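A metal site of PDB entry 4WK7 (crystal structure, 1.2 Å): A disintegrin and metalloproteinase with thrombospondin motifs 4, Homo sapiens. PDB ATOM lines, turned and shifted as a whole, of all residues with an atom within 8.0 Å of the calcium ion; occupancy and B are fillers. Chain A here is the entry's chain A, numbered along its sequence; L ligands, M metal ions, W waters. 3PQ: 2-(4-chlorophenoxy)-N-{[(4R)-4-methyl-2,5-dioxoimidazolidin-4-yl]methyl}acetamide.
The side-chain hydroxyl (OG1) of Thr 117 sits at hydrogen-bond distance from an oxygen (O12) of the ligand, 3.1 Å away. O12 of the ligand sits at hydrogen-bond distance from N of Leu 118, at 2.7 Å. O12 of the ligand sits at hydrogen-bond distance from N of Gly 119 (3.2 Å). A nitrogen (N4) of the ligand lies within hydrogen-bond range of the backbone carbonyl oxygen of Gly 119 (3.1 Å).
The side-chain sulfur of Cys 110 is disulfide-bonded to the side-chain sulfur of Cys 115. N of Glu 137 lies within hydrogen-bond range of O of Leu 118, at 2.7 Å. The side-chain hydroxyl (OG1) of Thr 117 sits at hydrogen-bond distance from the backbone carbonyl oxygen (O) of Gly 119 (3.1 Å).
OD1 of Asp 108 is bound to the calcium ion. O of Cys 115 binds the calcium ion. The calcium ion is bound by the backbone carbonyl oxygen (O) of Leu 109 (2.4 Å). The calcium ion is bound by OE1 of Glu 137 (2.4 Å). The calcium ion is bound by the backbone carbonyl oxygen (O) of Thr 117. Water W1 is bound to the calcium ion, at 2.4 Å. The calcium ion has six donor atoms within binding distance.
Within 4 Å of the calcium ion: Asp 108, Leu 109, Cys 115, Thr 117 and Glu 137.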
ATOM      1  N   PRO A  71      19.107  10.809 -20.155  1.00  0.00           N
ATOM      2  CA  PRO A  71      18.753  11.720 -19.071  1.00  0.00           C
ATOM      3  C   PRO A  71      19.380  11.379 -17.715  1.00  0.00           C
ATOM      4  O   PRO A  71      19.741  12.293 -16.977  1.00  0.00           O
ATOM      5  CB  PRO A  71      17.225  11.589 -18.983  1.00  0.00           C
ATOM      6  CG  PRO A  71      16.803  11.151 -20.341  1.00  0.00           C
ATOM      7  CD  PRO A  71      17.917  10.314 -20.880  1.00  0.00           C
ATOM      8  N   ALA A  73      21.939  10.918 -15.187  1.00  0.00           N
ATOM      9  CA  ALA A  73      23.349  11.278 -15.004  1.00  0.00           C
ATOM     10  C   ALA A  73      24.170  10.077 -14.540  1.00  0.00           C
ATOM     11  O   ALA A  73      25.257   9.847 -15.056  1.00  0.00           O
ATOM     12  CB  ALA A  73      23.476  12.426 -14.009  1.00  0.00           C
ATOM     13  N   ARG A 106      25.329  17.608 -24.851  1.00  0.00           N
ATOM     14  CA  ARG A 106      24.211  18.559 -24.849  1.00  0.00           C
ATOM     15  C   ARG A 106      22.975  17.947 -24.202  1.00  0.00           C
ATOM     16  O   ARG A 106      21.962  18.638 -24.014  1.00  0.00           O
ATOM     17  CB  ARG A 106      23.857  19.011 -26.273  1.00  0.00           C
ATOM     18  CG  ARG A 106      24.998  19.653 -27.048  1.00  0.00           C
ATOM     19  CD  ARG A 106      25.300  21.065 -26.578  1.00  0.00           C
ATOM     20  NE  ARG A 106      24.279  22.025 -26.999  1.00  0.00           N
ATOM     21  CZ  ARG A 106      24.321  23.328 -26.750  1.00  0.00           C
ATOM     22  NH1 ARG A 106      23.336  24.112 -27.184  1.00  0.00           N
ATOM     23  NH2 ARG A 106      25.325  23.855 -26.062  1.00  0.00           N
ATOM     24  N   GLN A 107      23.028  16.655 -23.860  1.00  0.00           N
ATOM     25  CA  GLN A 107      21.940  15.986 -23.147  1.00  0.00           C
ATOM     26  C   GLN A 107      21.665  16.679 -21.818  1.00  0.00           C
ATOM     27  O   GLN A 107      22.594  17.001 -21.077  1.00  0.00           O
ATOM     28  CB  GLN A 107      22.289  14.512 -22.895  1.00  0.00           C
ATOM     29  CG  GLN A 107      21.325  13.738 -22.001  1.00  0.00           C
ATOM     30  CD  GLN A 107      19.964  13.511 -22.642  1.00  0.00           C
ATOM     31  OE1 GLN A 107      19.873  13.026 -23.769  1.00  0.00           O
ATOM     32  NE2 GLN A 107      18.910  13.863 -21.921  1.00  0.00           N
ATOM     33  N   ASP A 108      20.390  16.921 -21.529  1.00  0.00           N
ATOM     34  CA  ASP A 108      19.964  17.420 -20.233  1.00  0.00           C
ATOM     35  C   ASP A 108      20.094  16.290 -19.220  1.00  0.00           C
ATOM     36  O   ASP A 108      19.286  15.346 -19.224  1.00  0.00           O
ATOM     37  CB  ASP A 108      18.522  17.944 -20.297  1.00  0.00           C
ATOM     38  CG  ASP A 108      18.062  18.595 -19.006  1.00  0.00           C
ATOM     39  OD1 ASP A 108      18.846  18.670 -18.028  1.00  0.00           O
ATOM     40  OD2 ASP A 108      16.899  19.051 -18.947  1.00  0.00           O
ATOM     41  N   LEU A 109      21.115  16.368 -18.382  1.00  0.00           N
ATOM     42  CA  LEU A 109      21.366  15.346 -17.371  1.00  0.00           C
ATOM     43  C   LEU A 109      20.471  15.554 -16.165  1.00  0.00           C
ATOM     44  O   LEU A 109      20.233  16.694 -15.748  1.00  0.00           O
ATOM     45  CB  LEU A 109      22.837  15.378 -16.932  1.00  0.00           C
ATOM     46  CG  LEU A 109      23.856  15.116 -18.042  1.00  0.00           C
ATOM     47  CD1 LEU A 109      25.272  15.335 -17.504  1.00  0.00           C
ATOM     48  CD2 LEU A 109      23.703  13.712 -18.614  1.00  0.00           C
ATOM     49  N   CYS A 110      19.982  14.460 -15.601  1.00  0.00           N
ATOM     50  CA  CYS A 110      19.013  14.511 -14.523  1.00  0.00           C
ATOM     51  C   CYS A 110      19.382  13.579 -13.376  1.00  0.00           C
ATOM     52  O   CYS A 110      20.121  12.597 -13.559  1.00  0.00           O
ATOM     53  CB  CYS A 110      17.614  14.158 -15.032  1.00  0.00           C
ATOM     54  SG  CYS A 110      17.111  14.998 -16.565  1.00  0.00           S
ATOM     55  N   GLY A 111      18.873  13.904 -12.187  1.00  0.00           N
ATOM     56  CA  GLY A 111      18.932  13.020 -11.038  1.00  0.00           C
ATOM     57  C   GLY A 111      17.603  12.314 -10.855  1.00  0.00           C
ATOM     58  O   GLY A 111      16.830  12.164 -11.800  1.00  0.00           O
ATOM     59  N   THR A 114      14.789  15.779 -10.264  1.00  0.00           N
ATOM     60  CA  THR A 114      14.887  16.955 -11.110  1.00  0.00           C
ATOM     61  C   THR A 114      15.953  16.772 -12.174  1.00  0.00           C
ATOM     62  O   THR A 114      16.728  15.811 -12.133  1.00  0.00           O
ATOM     63  CB  THR A 114      15.262  18.218 -10.289  1.00  0.00           C
ATOM     64  OG1 THR A 114      16.604  18.101  -9.807  1.00  0.00           O
ATOM     65  CG2 THR A 114      14.306  18.403  -9.121  1.00  0.00           C
ATOM     66  N   CYS A 115      15.977  17.695 -13.137  1.00  0.00           N
ATOM     67  CA  CYS A 115      17.032  17.753 -14.155  1.00  0.00           C
ATOM     68  C   CYS A 115      17.954  18.958 -13.943  1.00  0.00           C
ATOM     69  O   CYS A 115      18.616  19.404 -14.884  1.00  0.00           O
ATOM     70  CB  CYS A 115      16.411  17.770 -15.548  1.00  0.00           C
ATOM     71  SG  CYS A 115      15.593  16.229 -16.007  1.00  0.00           S
ATOM     72  N   ASP A 116      18.007  19.464 -12.713  1.00  0.00           N
ATOM     73  CA  ASP A 116      18.833  20.627 -12.399  1.00  0.00           C
ATOM     74  C   ASP A 116      20.330  20.343 -12.487  1.00  0.00           C
ATOM     75  O   ASP A 116      21.133  21.248 -12.698  1.00  0.00           O
ATOM     76  CB  ASP A 116      18.509  21.162 -10.996  1.00  0.00           C
ATOM     77  CG  ASP A 116      17.059  21.579 -10.850  1.00  0.00           C
ATOM     78  OD1 ASP A 116      16.435  21.963 -11.865  1.00  0.00           O
ATOM     79  OD2 ASP A 116      16.552  21.541  -9.710  1.00  0.00           O
ATOM     80  N   THR A 117      20.702  19.070 -12.318  1.00  0.00           N
ATOM     81  CA  THR A 117      22.114  18.698 -12.343  1.00  0.00           C
ATOM     82  C   THR A 117      22.750  19.033 -13.688  1.00  0.00           C
ATOM     83  O   THR A 117      22.114  18.969 -14.739  1.00  0.00           O
ATOM     84  CB  THR A 117      22.353  17.208 -11.976  1.00  0.00           C
ATOM     85  OG1 THR A 117      23.765  16.980 -11.843  1.00  0.00           O
ATOM     86  CG2 THR A 117      21.787  16.261 -13.031  1.00  0.00           C
ATOM     87  N   LEU A 118      24.025  19.418 -13.629  1.00  0.00           N
ATOM     88  CA  LEU A 118      24.804  19.741 -14.817  1.00  0.00           C
ATOM     89  C   LEU A 118      25.984  18.788 -15.031  1.00  0.00           C
ATOM     90  O   LEU A 118      26.735  18.948 -15.985  1.00  0.00           O
ATOM     91  CB  LEU A 118      25.339  21.175 -14.714  1.00  0.00           C
ATOM     92  CG  LEU A 118      24.283  22.281 -14.782  1.00  0.00           C
ATOM     93  CD1 LEU A 118      24.919  23.618 -14.426  1.00  0.00           C
ATOM     94  CD2 LEU A 118      23.644  22.339 -16.162  1.00  0.00           C
ATOM     95  N   GLY A 119      26.145  17.796 -14.165  1.00  0.00           N
ATOM     96  CA  GLY A 119      27.268  16.883 -14.318  1.00  0.00           C
ATOM     97  C   GLY A 119      27.382  15.903 -13.188  1.00  0.00           C
ATOM     98  O   GLY A 119      26.638  15.973 -12.206  1.00  0.00           O
ATOM     99  N   GLU A 137      27.173  18.417 -18.622  1.00  0.00           N
ATOM    100  CA  GLU A 137      26.151  18.970 -19.501  1.00  0.00           C
ATOM    101  C   GLU A 137      26.635  20.342 -19.968  1.00  0.00           C
ATOM    102  O   GLU A 137      26.795  21.242 -19.158  1.00  0.00           O
ATOM    103  CB  GLU A 137      24.830  19.120 -18.740  1.00  0.00           C
ATOM    104  CG  GLU A 137      23.733  19.783 -19.553  1.00  0.00           C
ATOM    105  CD  GLU A 137      22.441  19.921 -18.777  1.00  0.00           C
ATOM    106  OE1 GLU A 137      22.147  19.056 -17.922  1.00  0.00           O
ATOM    107  OE2 GLU A 137      21.710  20.905 -19.029  1.00  0.00           O
HETATM  108  C7  3PQ L   1      26.128  17.890  -7.253  1.00  0.00           C
HETATM  109  C6  3PQ L   1      24.251  16.647  -8.203  1.00  0.00           C
HETATM  110  N1  3PQ L   1      27.433  17.646  -7.587  1.00  0.00           N
HETATM  111  C5  3PQ L   1      25.315  17.688  -8.497  1.00  0.00           C
HETATM  112  C2  3PQ L   1      27.572  17.241  -8.875  1.00  0.00           C
HETATM  113  C16 3PQ L   1      28.764  23.418 -10.991  1.00  0.00           C
HETATM  114  C21 3PQ L   1      28.611  23.677  -8.626  1.00  0.00           C
HETATM  115  C17 3PQ L   1      29.621  24.507 -11.043  1.00  0.00           C
HETATM  116  C20 3PQ L   1      29.455  24.760  -8.689  1.00  0.00           C
HETATM  117  C13 3PQ L   1      27.066  21.280 -10.837  1.00  0.00           C
HETATM  118  C9  3PQ L   1      24.715  19.027  -8.899  1.00  0.00           C
HETATM  119  C15 3PQ L   1      28.261  23.000  -9.778  1.00  0.00           C
HETATM  120  C18 3PQ L   1      29.962  25.173  -9.894  1.00  0.00           C
HETATM  121  C11 3PQ L   1      26.101  20.151 -10.553  1.00  0.00           C
HETATM  122  N4  3PQ L   1      26.313  17.201  -9.408  1.00  0.00           N
HETATM  123  N10 3PQ L   1      25.731  19.997  -9.234  1.00  0.00           N
HETATM  124  O8  3PQ L   1      25.701  18.232  -6.165  1.00  0.00           O
HETATM  125  O3  3PQ L   1      28.643  16.966  -9.414  1.00  0.00           O
HETATM  126  O12 3PQ L   1      25.687  19.436 -11.441  1.00  0.00           O
HETATM  127  O14 3PQ L   1      27.397  21.922  -9.606  1.00  0.00           O
HETATM  128 CL1  3PQ L   1      31.030  26.547  -9.949  1.00  0.00          CL
HETATM  129 CA    CA M   1      20.360  18.981 -16.356  1.00  0.00          CA
HETATM  130  O   HOH W   1      20.190  21.362 -16.721  1.00  0.00           O
